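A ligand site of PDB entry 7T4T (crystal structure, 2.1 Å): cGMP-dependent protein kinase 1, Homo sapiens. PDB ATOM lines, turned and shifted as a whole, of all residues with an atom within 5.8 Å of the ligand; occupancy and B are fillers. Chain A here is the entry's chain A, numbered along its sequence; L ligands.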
ATOM      1  N   ILE A  47       7.515   7.620 -13.046  1.00  0.00           N
ATOM      2  CA  ILE A  47       6.105   7.673 -12.692  1.00  0.00           C
ATOM      3  C   ILE A  47       5.855   8.975 -11.928  1.00  0.00           C
ATOM      4  O   ILE A  47       6.681   9.344 -11.081  1.00  0.00           O
ATOM      5  CB  ILE A  47       5.715   6.427 -11.809  1.00  0.00           C
ATOM      6  CG1 ILE A  47       5.671   5.134 -12.650  1.00  0.00           C
ATOM      7  CG2 ILE A  47       4.381   6.667 -11.088  1.00  0.00           C
ATOM      8  CD1 ILE A  47       5.423   3.888 -11.809  1.00  0.00           C
ATOM      9  N   VAL A  66      11.471   6.803  -4.459  1.00  0.00           N
ATOM     10  CA  VAL A  66      10.014   6.745  -4.375  1.00  0.00           C
ATOM     11  C   VAL A  66       9.595   7.816  -3.319  1.00  0.00           C
ATOM     12  O   VAL A  66      10.084   7.791  -2.187  1.00  0.00           O
ATOM     13  CB  VAL A  66       9.472   5.340  -4.025  1.00  0.00           C
ATOM     14  CG1 VAL A  66       7.953   5.328  -4.102  1.00  0.00           C
ATOM     15  CG2 VAL A  66      10.079   4.280  -4.961  1.00  0.00           C
ATOM     16  N   ARG A  68       6.079  10.486  -2.036  1.00  0.00           N
ATOM     17  CA  ARG A  68       4.620  10.576  -2.057  1.00  0.00           C
ATOM     18  C   ARG A  68       4.186  11.835  -1.311  1.00  0.00           C
ATOM     19  O   ARG A  68       4.664  12.111  -0.207  1.00  0.00           O
ATOM     20  CB  ARG A  68       4.026   9.321  -1.405  1.00  0.00           C
ATOM     21  CG  ARG A  68       2.567   9.433  -1.038  1.00  0.00           C
ATOM     22  CD  ARG A  68       1.956   8.111  -0.648  1.00  0.00           C
ATOM     23  NE  ARG A  68       0.603   8.339  -0.138  1.00  0.00           N
ATOM     24  CZ  ARG A  68      -0.495   8.488  -0.890  1.00  0.00           C
ATOM     25  NH1 ARG A  68      -0.415   8.398  -2.219  1.00  0.00           N
ATOM     26  NH2 ARG A  68      -1.665   8.702  -0.319  1.00  0.00           N
ATOM     27  N   LEU A  79       9.924   7.750   0.652  1.00  0.00           N
ATOM     28  CA  LEU A  79       9.486   6.424   1.082  1.00  0.00           C
ATOM     29  C   LEU A  79      10.658   5.455   1.059  1.00  0.00           C
ATOM     30  O   LEU A  79      10.947   4.817   2.073  1.00  0.00           O
ATOM     31  CB  LEU A  79       8.351   5.910   0.180  1.00  0.00           C
ATOM     32  CG  LEU A  79       7.100   6.784   0.127  1.00  0.00           C
ATOM     33  CD1 LEU A  79       6.002   6.091  -0.631  1.00  0.00           C
ATOM     34  CD2 LEU A  79       6.624   7.168   1.509  1.00  0.00           C
ATOM     35  N   ARG A  80      11.287   5.291  -0.118  1.00  0.00           N
ATOM     36  CA  ARG A  80      12.380   4.364  -0.246  1.00  0.00           C
ATOM     37  C   ARG A  80      13.091   4.502  -1.590  1.00  0.00           C
ATOM     38  O   ARG A  80      12.514   5.046  -2.540  1.00  0.00           O
ATOM     39  CB  ARG A  80      11.877   2.891  -0.118  1.00  0.00           C
ATOM     40  CG  ARG A  80      10.617   2.628  -0.960  1.00  0.00           C
ATOM     41  CD  ARG A  80      10.494   1.161  -1.304  1.00  0.00           C
ATOM     42  NE  ARG A  80      10.254   0.336  -0.116  1.00  0.00           N
ATOM     43  CZ  ARG A  80       9.113  -0.275   0.212  1.00  0.00           C
ATOM     44  NH1 ARG A  80       8.032  -0.117  -0.528  1.00  0.00           N
ATOM     45  NH2 ARG A  80       9.039  -1.039   1.297  1.00  0.00           N
ATOM     46  N   LEU A  82      14.771   2.114  -4.606  1.00  0.00           N
ATOM     47  CA  LEU A  82      14.723   0.779  -5.202  1.00  0.00           C
ATOM     48  C   LEU A  82      15.920   0.647  -6.175  1.00  0.00           C
ATOM     49  O   LEU A  82      16.343   1.638  -6.766  1.00  0.00           O
ATOM     50  CB  LEU A  82      13.392   0.580  -5.958  1.00  0.00           C
ATOM     51  CG  LEU A  82      12.103   0.598  -5.148  1.00  0.00           C
ATOM     52  CD1 LEU A  82      10.923   0.518  -6.080  1.00  0.00           C
ATOM     53  CD2 LEU A  82      12.063  -0.554  -4.111  1.00  0.00           C
ATOM     54  N   TRP A  87      11.051  -3.934  -8.378  1.00  0.00           N
ATOM     55  CA  TRP A  87      10.001  -3.622  -9.323  1.00  0.00           C
ATOM     56  C   TRP A  87       8.973  -2.645  -8.721  1.00  0.00           C
ATOM     57  O   TRP A  87       8.934  -2.481  -7.516  1.00  0.00           O
ATOM     58  CB  TRP A  87       9.356  -4.896  -9.865  1.00  0.00           C
ATOM     59  CG  TRP A  87       9.192  -5.994  -8.858  1.00  0.00           C
ATOM     60  CD1 TRP A  87      10.009  -7.075  -8.673  1.00  0.00           C
ATOM     61  CD2 TRP A  87       8.101  -6.155  -7.952  1.00  0.00           C
ATOM     62  NE1 TRP A  87       9.534  -7.865  -7.655  1.00  0.00           N
ATOM     63  CE2 TRP A  87       8.340  -7.330  -7.210  1.00  0.00           C
ATOM     64  CE3 TRP A  87       6.929  -5.402  -7.680  1.00  0.00           C
ATOM     65  CZ2 TRP A  87       7.462  -7.789  -6.231  1.00  0.00           C
ATOM     66  CZ3 TRP A  87       6.079  -5.819  -6.680  1.00  0.00           C
ATOM     67  CH2 TRP A  87       6.339  -7.016  -5.979  1.00  0.00           C
ATOM     68  N   PHE A  88       8.194  -1.969  -9.590  1.00  0.00           N
ATOM     69  CA  PHE A  88       7.190  -0.999  -9.142  1.00  0.00           C
ATOM     70  C   PHE A  88       6.150  -0.757 -10.247  1.00  0.00           C
ATOM     71  O   PHE A  88       6.357  -1.162 -11.389  1.00  0.00           O
ATOM     72  CB  PHE A  88       7.851   0.345  -8.764  1.00  0.00           C
ATOM     73  CG  PHE A  88       8.682   0.972  -9.861  1.00  0.00           C
ATOM     74  CD1 PHE A  88      10.028   0.671  -9.980  1.00  0.00           C
ATOM     75  CD2 PHE A  88       8.128   1.848 -10.776  1.00  0.00           C
ATOM     76  CE1 PHE A  88      10.801   1.260 -10.967  1.00  0.00           C
ATOM     77  CE2 PHE A  88       8.901   2.415 -11.798  1.00  0.00           C
ATOM     78  CZ  PHE A  88      10.228   2.098 -11.900  1.00  0.00           C
ATOM     79  N   GLY A  89       5.060  -0.059  -9.874  1.00  0.00           N
ATOM     80  CA  GLY A  89       4.004   0.308 -10.804  1.00  0.00           C
ATOM     81  C   GLY A  89       2.835  -0.636 -10.843  1.00  0.00           C
ATOM     82  O   GLY A  89       1.928  -0.433 -11.639  1.00  0.00           O
ATOM     83  N   GLU A  90       2.782  -1.642  -9.972  1.00  0.00           N
ATOM     84  CA  GLU A  90       1.673  -2.608  -9.946  1.00  0.00           C
ATOM     85  C   GLU A  90       0.389  -2.116  -9.232  1.00  0.00           C
ATOM     86  O   GLU A  90      -0.676  -2.637  -9.521  1.00  0.00           O
ATOM     87  CB  GLU A  90       2.129  -3.977  -9.352  1.00  0.00           C
ATOM     88  CG  GLU A  90       2.141  -4.108  -7.828  1.00  0.00           C
ATOM     89  CD  GLU A  90       3.168  -3.299  -7.072  1.00  0.00           C
ATOM     90  OE1 GLU A  90       4.039  -2.677  -7.719  1.00  0.00           O
ATOM     91  OE2 GLU A  90       3.113  -3.301  -5.826  1.00  0.00           O
ATOM     92  N   LYS A  91       0.476  -1.144  -8.330  1.00  0.00           N
ATOM     93  CA  LYS A  91      -0.704  -0.654  -7.609  1.00  0.00           C
ATOM     94  C   LYS A  91      -1.811  -0.053  -8.530  1.00  0.00           C
ATOM     95  O   LYS A  91      -2.997  -0.285  -8.283  1.00  0.00           O
ATOM     96  CB  LYS A  91      -0.320   0.359  -6.526  1.00  0.00           C
ATOM     97  CG  LYS A  91       0.531  -0.210  -5.402  1.00  0.00           C
ATOM     98  CD  LYS A  91       0.841   0.877  -4.370  1.00  0.00           C
ATOM     99  CE  LYS A  91       1.286   0.312  -3.046  1.00  0.00           C
ATOM    100  NZ  LYS A  91       0.229   0.429  -2.001  1.00  0.00           N
ATOM    101  N   ALA A  92      -1.434   0.661  -9.606  1.00  0.00           N
ATOM    102  CA  ALA A  92      -2.380   1.254 -10.547  1.00  0.00           C
ATOM    103  C   ALA A  92      -3.020   0.180 -11.481  1.00  0.00           C
ATOM    104  O   ALA A  92      -3.984   0.472 -12.190  1.00  0.00           O
ATOM    105  CB  ALA A  92      -1.721   2.350 -11.364  1.00  0.00           C
ATOM    106  N   LEU A  93      -2.473  -1.047 -11.482  1.00  0.00           N
ATOM    107  CA  LEU A  93      -2.989  -2.174 -12.245  1.00  0.00           C
ATOM    108  C   LEU A  93      -3.817  -3.085 -11.308  1.00  0.00           C
ATOM    109  O   LEU A  93      -4.381  -4.062 -11.790  1.00  0.00           O
ATOM    110  CB  LEU A  93      -1.823  -2.992 -12.859  1.00  0.00           C
ATOM    111  CG  LEU A  93      -0.619  -2.208 -13.429  1.00  0.00           C
ATOM    112  CD1 LEU A  93       0.410  -3.147 -14.028  1.00  0.00           C
ATOM    113  CD2 LEU A  93      -1.062  -1.208 -14.463  1.00  0.00           C
ATOM    114  N   VAL A  98      -4.844   5.232 -10.721  1.00  0.00           N
ATOM    115  CA  VAL A  98      -4.039   6.392 -10.435  1.00  0.00           C
ATOM    116  C   VAL A  98      -2.713   5.953  -9.799  1.00  0.00           C
ATOM    117  O   VAL A  98      -2.686   5.027  -8.974  1.00  0.00           O
ATOM    118  CB  VAL A  98      -4.869   7.339  -9.488  1.00  0.00           C
ATOM    119  CG1 VAL A  98      -5.039   6.766  -8.078  1.00  0.00           C
ATOM    120  CG2 VAL A  98      -4.255   8.720  -9.427  1.00  0.00           C
ATOM    121  N   ARG A  99      -1.615   6.609 -10.199  1.00  0.00           N
ATOM    122  CA  ARG A  99      -0.302   6.332  -9.622  1.00  0.00           C
ATOM    123  C   ARG A  99      -0.313   6.913  -8.203  1.00  0.00           C
ATOM    124  O   ARG A  99      -0.778   8.042  -8.018  1.00  0.00           O
ATOM    125  CB  ARG A  99       0.804   6.960 -10.464  1.00  0.00           C
ATOM    126  CG  ARG A  99       0.898   6.364 -11.851  1.00  0.00           C
ATOM    127  CD  ARG A  99       1.313   4.908 -11.822  1.00  0.00           C
ATOM    128  NE  ARG A  99       1.780   4.480 -13.136  1.00  0.00           N
ATOM    129  CZ  ARG A  99       2.099   3.230 -13.462  1.00  0.00           C
ATOM    130  NH1 ARG A  99       2.004   2.251 -12.571  1.00  0.00           N
ATOM    131  NH2 ARG A  99       2.504   2.951 -14.687  1.00  0.00           N
ATOM    132  N   THR A 100       0.095   6.109  -7.205  1.00  0.00           N
ATOM    133  CA  THR A 100       0.025   6.477  -5.791  1.00  0.00           C
ATOM    134  C   THR A 100       1.334   7.071  -5.236  1.00  0.00           C
ATOM    135  O   THR A 100       1.381   7.394  -4.046  1.00  0.00           O
ATOM    136  CB  THR A 100      -0.425   5.249  -4.959  1.00  0.00           C
ATOM    137  OG1 THR A 100       0.613   4.276  -4.912  1.00  0.00           O
ATOM    138  CG2 THR A 100      -1.713   4.627  -5.468  1.00  0.00           C
ATOM    139  N   ALA A 101       2.362   7.232  -6.066  1.00  0.00           N
ATOM    140  CA  ALA A 101       3.644   7.759  -5.635  1.00  0.00           C
ATOM    141  C   ALA A 101       4.440   8.175  -6.838  1.00  0.00           C
ATOM    142  O   ALA A 101       4.098   7.784  -7.957  1.00  0.00           O
ATOM    143  CB  ALA A 101       4.422   6.671  -4.881  1.00  0.00           C
ATOM    144  N   ASN A 102       5.504   8.944  -6.627  1.00  0.00           N
ATOM    145  CA  ASN A 102       6.415   9.308  -7.733  1.00  0.00           C
ATOM    146  C   ASN A 102       7.597   8.354  -7.714  1.00  0.00           C
ATOM    147  O   ASN A 102       8.049   7.983  -6.637  1.00  0.00           O
ATOM    148  CB  ASN A 102       6.959  10.728  -7.548  1.00  0.00           C
ATOM    149  CG  ASN A 102       5.868  11.755  -7.393  1.00  0.00           C
ATOM    150  OD1 ASN A 102       5.213  12.097  -8.382  1.00  0.00           O
ATOM    151  ND2 ASN A 102       5.629  12.236  -6.172  1.00  0.00           N
ATOM    152  N   VAL A 103       8.117   7.965  -8.881  1.00  0.00           N
ATOM    153  CA  VAL A 103       9.321   7.130  -9.005  1.00  0.00           C
ATOM    154  C   VAL A 103      10.286   7.923  -9.884  1.00  0.00           C
ATOM    155  O   VAL A 103       9.996   8.194 -11.036  1.00  0.00           O
ATOM    156  CB  VAL A 103       9.068   5.676  -9.487  1.00  0.00           C
ATOM    157  CG1 VAL A 103      10.350   4.831  -9.335  1.00  0.00           C
ATOM    158  CG2 VAL A 103       7.924   5.042  -8.664  1.00  0.00           C
ATOM    159  N   GLU A 135       7.943  -4.323   2.642  1.00  0.00           N
ATOM    160  CA  GLU A 135       7.369  -3.898   3.904  1.00  0.00           C
ATOM    161  C   GLU A 135       6.665  -2.537   3.739  1.00  0.00           C
ATOM    162  O   GLU A 135       6.686  -1.967   2.641  1.00  0.00           O
ATOM    163  CB  GLU A 135       8.454  -3.866   4.999  1.00  0.00           C
ATOM    164  CG  GLU A 135       9.035  -5.249   5.259  1.00  0.00           C
ATOM    165  CD  GLU A 135       9.996  -5.377   6.419  1.00  0.00           C
ATOM    166  OE1 GLU A 135      10.372  -4.337   7.001  1.00  0.00           O
ATOM    167  OE2 GLU A 135      10.380  -6.526   6.752  1.00  0.00           O
ATOM    168  N   ASP A 136       6.015  -2.043   4.823  1.00  0.00           N
ATOM    169  CA  ASP A 136       5.265  -0.789   4.809  1.00  0.00           C
ATOM    170  C   ASP A 136       6.208   0.425   4.987  1.00  0.00           C
ATOM    171  O   ASP A 136       6.451   0.878   6.102  1.00  0.00           O
ATOM    172  CB  ASP A 136       4.154  -0.836   5.870  1.00  0.00           C
ATOM    173  CG  ASP A 136       3.050   0.202   5.734  1.00  0.00           C
ATOM    174  OD1 ASP A 136       3.253   1.192   5.009  1.00  0.00           O
ATOM    175  OD2 ASP A 136       2.007   0.037   6.385  1.00  0.00           O
ATOM    176  N   ALA A 137       6.711   0.959   3.870  1.00  0.00           N
ATOM    177  CA  ALA A 137       7.599   2.130   3.856  1.00  0.00           C
ATOM    178  C   ALA A 137       6.846   3.407   4.253  1.00  0.00           C
ATOM    179  O   ALA A 137       7.479   4.331   4.784  1.00  0.00           O
ATOM    180  CB  ALA A 137       8.246   2.296   2.477  1.00  0.00           C
ATOM    181  N   GLU A 138       5.512   3.480   3.970  1.00  0.00           N
ATOM    182  CA  GLU A 138       4.668   4.637   4.349  1.00  0.00           C
ATOM    183  C   GLU A 138       4.537   4.726   5.888  1.00  0.00           C
ATOM    184  O   GLU A 138       4.688   5.802   6.456  1.00  0.00           O
ATOM    185  CB  GLU A 138       3.284   4.547   3.694  1.00  0.00           C
ATOM    186  CG  GLU A 138       3.323   4.710   2.190  1.00  0.00           C
ATOM    187  CD  GLU A 138       1.969   4.595   1.522  1.00  0.00           C
ATOM    188  OE1 GLU A 138       0.935   4.831   2.190  1.00  0.00           O
ATOM    189  OE2 GLU A 138       1.940   4.252   0.314  1.00  0.00           O
HETATM  190  P1  LIG L   1       1.934   2.800  -8.523  1.00  0.00           P
HETATM  191  O1  LIG L   1       1.010   3.522  -7.609  1.00  0.00           O
HETATM  192  O2  LIG L   1       1.199   2.221  -9.687  1.00  0.00           O
HETATM  193  O3  LIG L   1       3.067   3.738  -9.093  1.00  0.00           O
HETATM  194  C1  LIG L   1       4.077   4.228  -8.154  1.00  0.00           C
HETATM  195  C2  LIG L   1       4.688   2.968  -7.600  1.00  0.00           C
HETATM  196  O4  LIG L   1       5.692   3.117  -6.581  1.00  0.00           O
HETATM  197  C3  LIG L   1       3.656   2.119  -6.874  1.00  0.00           C
HETATM  198  O5  LIG L   1       2.663   1.625  -7.782  1.00  0.00           O
HETATM  199  C4  LIG L   1       4.539   1.065  -6.191  1.00  0.00           C
HETATM  200  O6  LIG L   1       4.745  -0.073  -7.023  1.00  0.00           O
HETATM  201  C5  LIG L   1       5.842   1.860  -5.949  1.00  0.00           C
HETATM  202  N1  LIG L   1       6.113   2.076  -4.530  1.00  0.00           N
HETATM  203  C6  LIG L   1       7.222   1.646  -3.856  1.00  0.00           C
HETATM  204  N2  LIG L   1       7.166   1.869  -2.569  1.00  0.00           N
HETATM  205  C7  LIG L   1       5.926   2.437  -2.368  1.00  0.00           C
HETATM  206  C8  LIG L   1       5.257   2.832  -1.188  1.00  0.00           C
HETATM  207  O7  LIG L   1       5.729   2.794  -0.054  1.00  0.00           O
HETATM  208  N3  LIG L   1       4.005   3.364  -1.418  1.00  0.00           N
HETATM  209  C9  LIG L   1       3.424   3.478  -2.649  1.00  0.00           C
HETATM  210  N4  LIG L   1       2.205   4.027  -2.703  1.00  0.00           N
HETATM  211  N5  LIG L   1       4.014   3.077  -3.778  1.00  0.00           N
HETATM  212  C10 LIG L   1       5.260   2.579  -3.569  1.00  0.00           C
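The backbone carbonyl oxygen (O) of Thr 100 is in hydrogen-bond range of the guanidinium group (NH1) of Arg 68 (2.8 Å).
OD1 of Asp 136 sits close to N of Glu 138, 3.4 Å away.
NH1 of Arg 99 sits at hydrogen-bond distance from O of Gly 89 (2.8 Å).
O of Arg 80 is in hydrogen-bond range of N of Val 66, 2.8 Å away.
The guanidinium group (NH2) of Arg 80 is in hydrogen-bond range of the backbone carbonyl oxygen (O) of Glu 135 (2.9 Å).
The backbone NH of Leu 79 is in hydrogen-bond range of the backbone carbonyl oxygen of Val 66, 2.8 Å away.
The backbone carbonyl oxygen of Ile 47 lies within hydrogen-bond range of the backbone NH of Val 103, 3.0 Å away.
Ile 47 touches the ligand.
Val 66 touches the ligand.
CD1 of Leu 79 touches O7 of the ligand (3.4 Å).
Phe 88 touches the ligand (CA to O6, 3.4 Å).
Lys 91 touches the ligand.
Ala 101 touches the ligand (O to C1, 3.6 Å).
Val 103 touches the ligand (CG2 to O4, 3.6 Å).
CB of Ala 137 touches O7 of the ligand (3.6 Å).
15 residues have an atom within 4 Å of the ligand: Ile 47, Val 66, Leu 79, Arg 80, Phe 88, Gly 89, Glu 90, Lys 91, Ala 92, Arg 99, Thr 100, Ala 101, Val 103, Ala 137 and Glu 138.
N of Thr 100 is in hydrogen-bond range of O1 of the ligand (2.8 Å).
The side-chain hydroxyl (OG1) of Thr 100 sits at hydrogen-bond distance from a nitrogen (N4) of the ligand (2.7 Å).
The side-chain carboxylate (OE1) of Glu 90 sits at hydrogen-bond distance from an oxygen (O6) of the ligand.
The side-chain carboxylate of Glu 138 lies within hydrogen-bond range of a nitrogen (N3) of the ligand, at 2.8 Å.
The backbone NH (N) of Gly 89 lies within hydrogen-bond range of an oxygen (O6) of the ligand (2.9 Å).
A nitrogen (N2) of the ligand lies within hydrogen-bond range of the guanidinium group (NH1) of Arg 80.
NH1 of Arg 99 is in salt-bridge range of O2 of the ligand, 3.0 Å away.
The backbone NH of Ala 92 sits at hydrogen-bond distance from an oxygen (O2) of the ligand.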
